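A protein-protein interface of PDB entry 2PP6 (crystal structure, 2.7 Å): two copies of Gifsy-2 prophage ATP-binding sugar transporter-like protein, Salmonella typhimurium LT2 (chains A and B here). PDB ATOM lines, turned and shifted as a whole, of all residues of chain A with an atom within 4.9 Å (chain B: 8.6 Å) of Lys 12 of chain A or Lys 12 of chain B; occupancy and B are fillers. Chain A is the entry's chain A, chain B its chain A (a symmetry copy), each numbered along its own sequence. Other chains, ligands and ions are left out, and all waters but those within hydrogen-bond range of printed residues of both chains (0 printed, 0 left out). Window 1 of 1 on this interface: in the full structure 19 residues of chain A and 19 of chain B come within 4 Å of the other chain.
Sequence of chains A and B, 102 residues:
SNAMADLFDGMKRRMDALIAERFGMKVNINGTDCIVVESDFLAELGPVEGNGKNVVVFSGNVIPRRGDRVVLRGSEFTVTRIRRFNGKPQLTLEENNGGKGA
NZ of Lys 88 of chain B lies within salt-bridge range of OD2 of Asp 16 of chain B, at 3.3 Å.
Asp 9 of chain A touches Asn 86 of chain B, and with the chains exchanged Asn 86 of chain A touches Asp 9 of chain B.
Lys 12 of chain A touches Met 15 of chain B, and with the chains exchanged Met 15 of chain A touches Lys 12 of chain B.
Lys 12 of chain A touches Asn 86 of chain B, and with the chains exchanged Asn 86 of chain A touches Lys 12 of chain B.
Asn 86 of chain A touches its own counterpart, Asn 86 of chain B.
10 positions are printed for both chains.
Of the 17 pairs that touch across the chains among the printed residues, 15 have their exchanged pair printed and touching as well.
The side-chain amino group of Lys 12 of chain B sits close to the backbone carbonyl oxygen of Lys 12 of chain A (3.5 Å).
NZ of Lys 12 of chain A lies within salt-bridge range of OD1 of Asp 16 of chain B, at 3.4 Å.
The side-chain carboxylate of Asp 16 of chain A lies within salt-bridge range of the side-chain amino group of Lys 12 of chain B (3.4 Å).
Printed residues of chain B within 4 Å of Asp 9 of chain A: Asn 86.
Of chain B, only Lys 12 (3.4 Å), Met 15 (3.6 Å), Asp 16 (3.4 Å) and Asn 86 (3.9 Å) come within 4 Å of Lys 12 of chain A.
Printed residues of chain A within 4 Å of Asp 9 of chain B: Asn 86.
Printed residues of chain A within 4 Å of Asn 86 of chain B: Asp 9 (3.7 Å), Lys 12 (3.9 Å) and Asn 86 (3.99 Å).
The nearest residue of chain B that does not touch Lys 12 of chain A is Met 11 of chain B (4.9 Å).
The nearest printed residue of chain A that does not touch Lys 12 of chain B is Met 11 of chain A (4.9 Å).
Hydrophobic or aromatic side chains of chain A within 4 Å of the printed part of chain B: Phe 8, Met 11 and Met 15.
Among the printed residues, 17 pairs touch across the chains.
Among the printed residues, merely in contact across the chains: Met 15 of chain A with Phe 8 of chain B (3.1 Å), Phe 8 of chain A with Met 15 of chain B (3.1 Å), Met 15 of chain A with Met 11 of chain B (3.3 Å), Met 11 of chain A with Met 15 of chain B (3.3 Å), Lys 12 of chain A with Met 15 of chain B (3.6 Å), Met 15 of chain A with Lys 12 of chain B (3.6 Å), Asp 9 of chain A with Asn 86 of chain B (3.7 Å), Asn 86 of chain A with Asp 9 of chain B (3.7 Å), Phe 8 of chain A with Ile 19 of chain B (3.7 Å), Met 11 of chain A with Met 11 of chain B (3.7 Å), Phe 8 of chain A with Leu 18 of chain B (3.9 Å), Asn 86 of chain A with Lys 12 of chain B (3.9 Å), Lys 12 of chain A with Asn 86 of chain B (3.9 Å) and Asn 86 of chain A with Asn 86 of chain B (3.99 Å).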
ATOM      1  N   PHE A   8     -18.452   3.987   8.366  1.00  0.00           N
ATOM      2  CA  PHE A   8     -18.289   3.735   6.939  1.00  0.00           C
ATOM      3  C   PHE A   8     -19.007   2.469   6.498  1.00  0.00           C
ATOM      4  O   PHE A   8     -19.613   2.437   5.424  1.00  0.00           O
ATOM      5  CB  PHE A   8     -16.806   3.624   6.585  1.00  0.00           C
ATOM      6  CG  PHE A   8     -16.085   4.949   6.535  1.00  0.00           C
ATOM      7  CD1 PHE A   8     -16.650   6.094   7.089  1.00  0.00           C
ATOM      8  CD2 PHE A   8     -14.832   5.046   5.938  1.00  0.00           C
ATOM      9  CE1 PHE A   8     -15.984   7.315   7.043  1.00  0.00           C
ATOM     10  CE2 PHE A   8     -14.163   6.262   5.891  1.00  0.00           C
ATOM     11  CZ  PHE A   8     -14.743   7.401   6.447  1.00  0.00           C
ATOM     12  N   ASP A   9     -18.953   1.433   7.333  1.00  0.00           N
ATOM     13  CA  ASP A   9     -19.600   0.176   6.986  1.00  0.00           C
ATOM     14  C   ASP A   9     -21.115   0.337   6.885  1.00  0.00           C
ATOM     15  O   ASP A   9     -21.745  -0.153   5.937  1.00  0.00           O
ATOM     16  CB  ASP A   9     -19.265  -0.901   8.015  1.00  0.00           C
ATOM     17  CG  ASP A   9     -19.590  -2.297   7.515  1.00  0.00           C
ATOM     18  OD1 ASP A   9     -18.900  -2.771   6.578  1.00  0.00           O
ATOM     19  OD2 ASP A   9     -20.536  -2.914   8.052  1.00  0.00           O
ATOM     20  N   GLY A  10     -21.688   1.029   7.867  1.00  0.00           N
ATOM     21  CA  GLY A  10     -23.119   1.258   7.880  1.00  0.00           C
ATOM     22  C   GLY A  10     -23.557   2.118   6.710  1.00  0.00           C
ATOM     23  O   GLY A  10     -24.623   1.919   6.141  1.00  0.00           O
ATOM     24  N   MET A  11     -22.740   3.087   6.333  1.00  0.00           N
ATOM     25  CA  MET A  11     -23.121   3.925   5.223  1.00  0.00           C
ATOM     26  C   MET A  11     -23.128   3.077   3.966  1.00  0.00           C
ATOM     27  O   MET A  11     -24.066   3.145   3.171  1.00  0.00           O
ATOM     28  CB  MET A  11     -22.166   5.106   5.124  1.00  0.00           C
ATOM     29  CG  MET A  11     -22.342   6.052   6.296  1.00  0.00           C
ATOM     30  SD  MET A  11     -21.251   7.620   6.247  1.00  0.00           S
ATOM     31  CE  MET A  11     -21.310   7.969   4.357  1.00  0.00           C
ATOM     32  N   LYS A  12     -22.099   2.255   3.799  1.00  0.00           N
ATOM     33  CA  LYS A  12     -22.047   1.380   2.638  1.00  0.00           C
ATOM     34  C   LYS A  12     -23.264   0.453   2.650  1.00  0.00           C
ATOM     35  O   LYS A  12     -23.932   0.290   1.640  1.00  0.00           O
ATOM     36  CB  LYS A  12     -20.764   0.546   2.634  1.00  0.00           C
ATOM     37  CG  LYS A  12     -19.484   1.366   2.540  1.00  0.00           C
ATOM     38  CD  LYS A  12     -18.253   0.476   2.624  1.00  0.00           C
ATOM     39  CE  LYS A  12     -16.975   1.294   2.699  1.00  0.00           C
ATOM     40  NZ  LYS A  12     -16.820   2.186   1.518  1.00  0.00           N
ATOM     41  N   ARG A  13     -23.575  -0.147   3.793  1.00  0.00           N
ATOM     42  CA  ARG A  13     -24.716  -1.041   3.827  1.00  0.00           C
ATOM     43  C   ARG A  13     -26.013  -0.330   3.422  1.00  0.00           C
ATOM     44  O   ARG A  13     -26.792  -0.864   2.630  1.00  0.00           O
ATOM     45  CB  ARG A  13     -24.871  -1.676   5.208  1.00  0.00           C
ATOM     46  CG  ARG A  13     -25.112  -3.179   5.146  1.00  0.00           C
ATOM     47  CD  ARG A  13     -26.008  -3.697   6.278  1.00  0.00           C
ATOM     48  NE  ARG A  13     -25.498  -3.388   7.615  1.00  0.00           N
ATOM     49  CZ  ARG A  13     -25.733  -2.254   8.271  1.00  0.00           C
ATOM     50  NH1 ARG A  13     -26.482  -1.301   7.722  1.00  0.00           N
ATOM     51  NH2 ARG A  13     -25.210  -2.069   9.477  1.00  0.00           N
ATOM     52  N   ARG A  14     -26.243   0.869   3.950  1.00  0.00           N
ATOM     53  CA  ARG A  14     -27.448   1.621   3.622  1.00  0.00           C
ATOM     54  C   ARG A  14     -27.413   2.103   2.164  1.00  0.00           C
ATOM     55  O   ARG A  14     -28.441   2.130   1.480  1.00  0.00           O
ATOM     56  CB  ARG A  14     -27.608   2.811   4.571  1.00  0.00           C
ATOM     57  CG  ARG A  14     -27.553   2.439   6.052  1.00  0.00           C
ATOM     58  CD  ARG A  14     -28.057   3.578   6.940  1.00  0.00           C
ATOM     59  NE  ARG A  14     -27.629   3.443   8.331  1.00  0.00           N
ATOM     60  CZ  ARG A  14     -26.377   3.631   8.746  1.00  0.00           C
ATOM     61  NH1 ARG A  14     -26.065   3.485  10.028  1.00  0.00           N
ATOM     62  NH2 ARG A  14     -25.435   3.972   7.881  1.00  0.00           N
ATOM     63  N   MET A  15     -26.232   2.473   1.678  1.00  0.00           N
ATOM     64  CA  MET A  15     -26.106   2.922   0.301  1.00  0.00           C
ATOM     65  C   MET A  15     -26.527   1.850  -0.696  1.00  0.00           C
ATOM     66  O   MET A  15     -27.194   2.141  -1.684  1.00  0.00           O
ATOM     67  CB  MET A  15     -24.672   3.348   0.014  1.00  0.00           C
ATOM     68  CG  MET A  15     -24.291   4.648   0.703  1.00  0.00           C
ATOM     69  SD  MET A  15     -22.492   5.220   0.364  1.00  0.00           S
ATOM     70  CE  MET A  15     -22.867   6.659  -0.815  1.00  0.00           C
ATOM     71  N   ASP A  16     -26.141   0.607  -0.448  1.00  0.00           N
ATOM     72  CA  ASP A  16     -26.496  -0.449  -1.368  1.00  0.00           C
ATOM     73  C   ASP A  16     -27.954  -0.815  -1.289  1.00  0.00           C
ATOM     74  O   ASP A  16     -28.573  -1.166  -2.294  1.00  0.00           O
ATOM     75  CB  ASP A  16     -25.671  -1.691  -1.104  1.00  0.00           C
ATOM     76  CG  ASP A  16     -24.232  -1.504  -1.461  1.00  0.00           C
ATOM     77  OD1 ASP A  16     -23.943  -0.632  -2.312  1.00  0.00           O
ATOM     78  OD2 ASP A  16     -23.391  -2.237  -0.901  1.00  0.00           O
ATOM     79  N   ASN A  86     -17.557  -4.581  -6.141  1.00  0.00           N
ATOM     80  CA  ASN A  86     -17.564  -4.161  -4.749  1.00  0.00           C
ATOM     81  C   ASN A  86     -18.017  -5.343  -3.909  1.00  0.00           C
ATOM     82  O   ASN A  86     -18.856  -5.208  -3.010  1.00  0.00           O
ATOM     83  CB  ASN A  86     -18.506  -2.979  -4.550  1.00  0.00           C
ATOM     84  CG  ASN A  86     -18.161  -1.812  -5.446  1.00  0.00           C
ATOM     85  OD1 ASN A  86     -18.186  -1.924  -6.671  1.00  0.00           O
ATOM     86  ND2 ASN A  86     -17.821  -0.686  -4.841  1.00  0.00           N
ATOM     87  N   MET B   4     -26.883   9.035  -8.820  1.00  0.00           N
ATOM     88  CA  MET B   4     -26.839   8.501  -7.474  1.00  0.00           C
ATOM     89  C   MET B   4     -25.820   7.364  -7.368  1.00  0.00           C
ATOM     90  O   MET B   4     -24.972   7.362  -6.470  1.00  0.00           O
ATOM     91  CB  MET B   4     -28.207   7.986  -7.045  1.00  0.00           C
ATOM     92  CG  MET B   4     -28.189   7.503  -5.621  1.00  0.00           C
ATOM     93  SD  MET B   4     -29.904   7.063  -4.892  1.00  0.00           S
ATOM     94  CE  MET B   4     -29.701   5.133  -4.788  1.00  0.00           C
ATOM     95  N   ALA B   5     -25.897   6.403  -8.284  1.00  0.00           N
ATOM     96  CA  ALA B   5     -24.978   5.273  -8.267  1.00  0.00           C
ATOM     97  C   ALA B   5     -23.515   5.696  -8.438  1.00  0.00           C
ATOM     98  O   ALA B   5     -22.633   5.165  -7.759  1.00  0.00           O
ATOM     99  CB  ALA B   5     -25.372   4.263  -9.344  1.00  0.00           C
ATOM    100  N   ASP B   6     -23.248   6.643  -9.336  1.00  0.00           N
ATOM    101  CA  ASP B   6     -21.875   7.112  -9.548  1.00  0.00           C
ATOM    102  C   ASP B   6     -21.363   7.845  -8.312  1.00  0.00           C
ATOM    103  O   ASP B   6     -20.166   7.823  -8.003  1.00  0.00           O
ATOM    104  CB  ASP B   6     -21.787   8.065 -10.749  1.00  0.00           C
ATOM    105  CG  ASP B   6     -21.806   7.341 -12.080  1.00  0.00           C
ATOM    106  OD1 ASP B   6     -21.014   6.388 -12.253  1.00  0.00           O
ATOM    107  OD2 ASP B   6     -22.606   7.735 -12.959  1.00  0.00           O
ATOM    108  N   LEU B   7     -22.274   8.506  -7.610  1.00  0.00           N
ATOM    109  CA  LEU B   7     -21.902   9.238  -6.416  1.00  0.00           C
ATOM    110  C   LEU B   7     -21.517   8.225  -5.357  1.00  0.00           C
ATOM    111  O   LEU B   7     -20.445   8.319  -4.769  1.00  0.00           O
ATOM    112  CB  LEU B   7     -23.077  10.081  -5.920  1.00  0.00           C
ATOM    113  CG  LEU B   7     -22.818  11.223  -4.933  1.00  0.00           C
ATOM    114  CD1 LEU B   7     -23.968  11.277  -3.936  1.00  0.00           C
ATOM    115  CD2 LEU B   7     -21.503  11.019  -4.208  1.00  0.00           C
ATOM    116  N   PHE B   8     -22.397   7.255  -5.130  1.00  0.00           N
ATOM    117  CA  PHE B   8     -22.170   6.219  -4.128  1.00  0.00           C
ATOM    118  C   PHE B   8     -20.850   5.496  -4.345  1.00  0.00           C
ATOM    119  O   PHE B   8     -20.141   5.189  -3.383  1.00  0.00           O
ATOM    120  CB  PHE B   8     -23.313   5.203  -4.147  1.00  0.00           C
ATOM    121  CG  PHE B   8     -24.583   5.693  -3.497  1.00  0.00           C
ATOM    122  CD1 PHE B   8     -24.773   7.045  -3.225  1.00  0.00           C
ATOM    123  CD2 PHE B   8     -25.594   4.797  -3.163  1.00  0.00           C
ATOM    124  CE1 PHE B   8     -25.945   7.496  -2.626  1.00  0.00           C
ATOM    125  CE2 PHE B   8     -26.766   5.243  -2.567  1.00  0.00           C
ATOM    126  CZ  PHE B   8     -26.941   6.600  -2.298  1.00  0.00           C
ATOM    127  N   ASP B   9     -20.513   5.239  -5.607  1.00  0.00           N
ATOM    128  CA  ASP B   9     -19.273   4.538  -5.907  1.00  0.00           C
ATOM    129  C   ASP B   9     -18.053   5.353  -5.483  1.00  0.00           C
ATOM    130  O   ASP B   9     -17.114   4.823  -4.873  1.00  0.00           O
ATOM    131  CB  ASP B   9     -19.185   4.218  -7.398  1.00  0.00           C
ATOM    132  CG  ASP B   9     -18.123   3.178  -7.704  1.00  0.00           C
ATOM    133  OD1 ASP B   9     -18.312   2.000  -7.313  1.00  0.00           O
ATOM    134  OD2 ASP B   9     -17.099   3.541  -8.325  1.00  0.00           O
ATOM    135  N   GLY B  10     -18.081   6.643  -5.810  1.00  0.00           N
ATOM    136  CA  GLY B  10     -16.986   7.524  -5.456  1.00  0.00           C
ATOM    137  C   GLY B  10     -16.853   7.673  -3.953  1.00  0.00           C
ATOM    138  O   GLY B  10     -15.754   7.764  -3.419  1.00  0.00           O
ATOM    139  N   MET B  11     -17.971   7.698  -3.247  1.00  0.00           N
ATOM    140  CA  MET B  11     -17.885   7.837  -1.814  1.00  0.00           C
ATOM    141  C   MET B  11     -17.242   6.584  -1.252  1.00  0.00           C
ATOM    142  O   MET B  11     -16.349   6.664  -0.408  1.00  0.00           O
ATOM    143  CB  MET B  11     -19.274   8.086  -1.242  1.00  0.00           C
ATOM    144  CG  MET B  11     -19.796   9.449  -1.651  1.00  0.00           C
ATOM    145  SD  MET B  11     -21.504   9.916  -0.929  1.00  0.00           S
ATOM    146  CE  MET B  11     -21.315   9.137   0.818  1.00  0.00           C
ATOM    147  N   LYS B  12     -17.672   5.426  -1.740  1.00  0.00           N
ATOM    148  CA  LYS B  12     -17.082   4.178  -1.280  1.00  0.00           C
ATOM    149  C   LYS B  12     -15.585   4.182  -1.598  1.00  0.00           C
ATOM    150  O   LYS B  12     -14.768   3.854  -0.749  1.00  0.00           O
ATOM    151  CB  LYS B  12     -17.747   2.974  -1.950  1.00  0.00           C
ATOM    152  CG  LYS B  12     -19.230   2.823  -1.635  1.00  0.00           C
ATOM    153  CD  LYS B  12     -19.839   1.657  -2.399  1.00  0.00           C
ATOM    154  CE  LYS B  12     -21.346   1.598  -2.222  1.00  0.00           C
ATOM    155  NZ  LYS B  12     -21.731   1.463  -0.791  1.00  0.00           N
ATOM    156  N   ARG B  13     -15.210   4.568  -2.810  1.00  0.00           N
ATOM    157  CA  ARG B  13     -13.797   4.568  -3.140  1.00  0.00           C
ATOM    158  C   ARG B  13     -12.989   5.472  -2.201  1.00  0.00           C
ATOM    159  O   ARG B  13     -11.928   5.074  -1.718  1.00  0.00           O
ATOM    160  CB  ARG B  13     -13.577   4.984  -4.594  1.00  0.00           C
ATOM    161  CG  ARG B  13     -12.604   4.071  -5.331  1.00  0.00           C
ATOM    162  CD  ARG B  13     -11.772   4.802  -6.392  1.00  0.00           C
ATOM    163  NE  ARG B  13     -12.583   5.486  -7.401  1.00  0.00           N
ATOM    164  CZ  ARG B  13     -13.065   6.720  -7.274  1.00  0.00           C
ATOM    165  NH1 ARG B  13     -12.819   7.429  -6.176  1.00  0.00           N
ATOM    166  NH2 ARG B  13     -13.803   7.244  -8.246  1.00  0.00           N
ATOM    167  N   ARG B  14     -13.487   6.676  -1.935  1.00  0.00           N
ATOM    168  CA  ARG B  14     -12.791   7.604  -1.052  1.00  0.00           C
ATOM    169  C   ARG B  14     -12.820   7.104   0.400  1.00  0.00           C
ATOM    170  O   ARG B  14     -11.848   7.263   1.146  1.00  0.00           O
ATOM    171  CB  ARG B  14     -13.413   8.998  -1.147  1.00  0.00           C
ATOM    172  CG  ARG B  14     -13.518   9.539  -2.572  1.00  0.00           C
ATOM    173  CD  ARG B  14     -13.815  11.039  -2.587  1.00  0.00           C
ATOM    174  NE  ARG B  14     -14.341  11.500  -3.871  1.00  0.00           N
ATOM    175  CZ  ARG B  14     -15.565  11.222  -4.316  1.00  0.00           C
ATOM    176  NH1 ARG B  14     -15.969  11.674  -5.497  1.00  0.00           N
ATOM    177  NH2 ARG B  14     -16.391  10.498  -3.576  1.00  0.00           N
ATOM    178  N   MET B  15     -13.927   6.487   0.804  1.00  0.00           N
ATOM    179  CA  MET B  15     -14.029   5.964   2.157  1.00  0.00           C
ATOM    180  C   MET B  15     -12.967   4.914   2.453  1.00  0.00           C
ATOM    181  O   MET B  15     -12.383   4.900   3.532  1.00  0.00           O
ATOM    182  CB  MET B  15     -15.412   5.366   2.387  1.00  0.00           C
ATOM    183  CG  MET B  15     -16.505   6.419   2.476  1.00  0.00           C
ATOM    184  SD  MET B  15     -18.261   5.706   2.769  1.00  0.00           S
ATOM    185  CE  MET B  15     -18.473   6.203   4.587  1.00  0.00           C
ATOM    186  N   ASP B  16     -12.708   4.030   1.501  1.00  0.00           N
ATOM    187  CA  ASP B  16     -11.722   2.998   1.731  1.00  0.00           C
ATOM    188  C   ASP B  16     -10.315   3.534   1.708  1.00  0.00           C
ATOM    189  O   ASP B  16      -9.446   3.059   2.440  1.00  0.00           O
ATOM    190  CB  ASP B  16     -11.839   1.902   0.695  1.00  0.00           C
ATOM    191  CG  ASP B  16     -13.093   1.105   0.849  1.00  0.00           C
ATOM    192  OD1 ASP B  16     -13.636   1.070   1.977  1.00  0.00           O
ATOM    193  OD2 ASP B  16     -13.530   0.501  -0.153  1.00  0.00           O
ATOM    194  N   ALA B  17     -10.080   4.523   0.863  1.00  0.00           N
ATOM    195  CA  ALA B  17      -8.749   5.080   0.762  1.00  0.00           C
ATOM    196  C   ALA B  17      -8.368   5.776   2.050  1.00  0.00           C
ATOM    197  O   ALA B  17      -7.190   5.849   2.394  1.00  0.00           O
ATOM    198  CB  ALA B  17      -8.676   6.045  -0.399  1.00  0.00           C
ATOM    199  N   LEU B  18      -9.370   6.277   2.765  1.00  0.00           N
ATOM    200  CA  LEU B  18      -9.129   6.979   4.013  1.00  0.00           C
ATOM    201  C   LEU B  18      -8.828   5.987   5.123  1.00  0.00           C
ATOM    202  O   LEU B  18      -7.946   6.222   5.952  1.00  0.00           O
ATOM    203  CB  LEU B  18     -10.343   7.836   4.376  1.00  0.00           C
ATOM    204  CG  LEU B  18     -10.281   8.668   5.659  1.00  0.00           C
ATOM    205  CD1 LEU B  18      -9.056   9.560   5.665  1.00  0.00           C
ATOM    206  CD2 LEU B  18     -11.546   9.496   5.761  1.00  0.00           C
ATOM    207  N   ILE B  19      -9.564   4.883   5.147  1.00  0.00           N
ATOM    208  CA  ILE B  19      -9.328   3.871   6.162  1.00  0.00           C
ATOM    209  C   ILE B  19      -7.923   3.313   5.985  1.00  0.00           C
ATOM    210  O   ILE B  19      -7.203   3.096   6.963  1.00  0.00           O
ATOM    211  CB  ILE B  19     -10.312   2.703   6.059  1.00  0.00           C
ATOM    212  CG1 ILE B  19     -11.705   3.149   6.478  1.00  0.00           C
ATOM    213  CG2 ILE B  19      -9.848   1.562   6.955  1.00  0.00           C
ATOM    214  CD1 ILE B  19     -12.678   2.008   6.549  1.00  0.00           C
ATOM    215  N   PHE B  58      -6.008  -3.852   1.060  1.00  0.00           N
ATOM    216  CA  PHE B  58      -6.534  -2.689   0.356  1.00  0.00           C
ATOM    217  C   PHE B  58      -5.901  -2.371  -0.993  1.00  0.00           C
ATOM    218  O   PHE B  58      -6.583  -1.900  -1.894  1.00  0.00           O
ATOM    219  CB  PHE B  58      -6.473  -1.465   1.258  1.00  0.00           C
ATOM    220  CG  PHE B  58      -7.591  -1.405   2.267  1.00  0.00           C
ATOM    221  CD1 PHE B  58      -8.533  -0.395   2.215  1.00  0.00           C
ATOM    222  CD2 PHE B  58      -7.705  -2.374   3.264  1.00  0.00           C
ATOM    223  CE1 PHE B  58      -9.579  -0.349   3.142  1.00  0.00           C
ATOM    224  CE2 PHE B  58      -8.743  -2.332   4.194  1.00  0.00           C
ATOM    225  CZ  PHE B  58      -9.682  -1.323   4.135  1.00  0.00           C
ATOM    226  N   PHE B  85     -14.406  -9.238   2.255  1.00  0.00           N
ATOM    227  CA  PHE B  85     -14.847  -8.189   3.145  1.00  0.00           C
ATOM    228  C   PHE B  85     -15.142  -7.030   2.219  1.00  0.00           C
ATOM    229  O   PHE B  85     -14.237  -6.299   1.815  1.00  0.00           O
ATOM    230  CB  PHE B  85     -13.750  -7.812   4.130  1.00  0.00           C
ATOM    231  CG  PHE B  85     -14.198  -6.838   5.164  1.00  0.00           C
ATOM    232  CD1 PHE B  85     -14.863  -7.275   6.298  1.00  0.00           C
ATOM    233  CD2 PHE B  85     -13.982  -5.474   4.993  1.00  0.00           C
ATOM    234  CE1 PHE B  85     -15.312  -6.366   7.259  1.00  0.00           C
ATOM    235  CE2 PHE B  85     -14.425  -4.555   5.941  1.00  0.00           C
ATOM    236  CZ  PHE B  85     -15.094  -5.004   7.080  1.00  0.00           C
ATOM    237  N   ASN B  86     -16.418  -6.885   1.871  1.00  0.00           N
ATOM    238  CA  ASN B  86     -16.856  -5.835   0.965  1.00  0.00           C
ATOM    239  C   ASN B  86     -16.016  -5.931  -0.297  1.00  0.00           C
ATOM    240  O   ASN B  86     -15.523  -4.923  -0.819  1.00  0.00           O
ATOM    241  CB  ASN B  86     -16.687  -4.464   1.609  1.00  0.00           C
ATOM    242  CG  ASN B  86     -17.418  -4.355   2.927  1.00  0.00           C
ATOM    243  OD1 ASN B  86     -17.136  -5.092   3.871  1.00  0.00           O
ATOM    244  ND2 ASN B  86     -18.374  -3.445   2.996  1.00  0.00           N
ATOM    245  N   LYS B  88     -13.050  -7.249  -0.641  1.00  0.00           N
ATOM    246  CA  LYS B  88     -11.609  -7.238  -0.471  1.00  0.00           C
ATOM    247  C   LYS B  88     -11.128  -8.489   0.211  1.00  0.00           C
ATOM    248  O   LYS B  88     -11.779  -9.045   1.084  1.00  0.00           O
ATOM    249  CB  LYS B  88     -11.158  -6.036   0.332  1.00  0.00           C
ATOM    250  CG  LYS B  88     -11.497  -4.751  -0.328  1.00  0.00           C
ATOM    251  CD  LYS B  88     -10.717  -3.634   0.287  1.00  0.00           C
ATOM    252  CE  LYS B  88     -11.479  -2.353   0.164  1.00  0.00           C
ATOM    253  NZ  LYS B  88     -12.759  -2.508   0.914  1.00  0.00           N
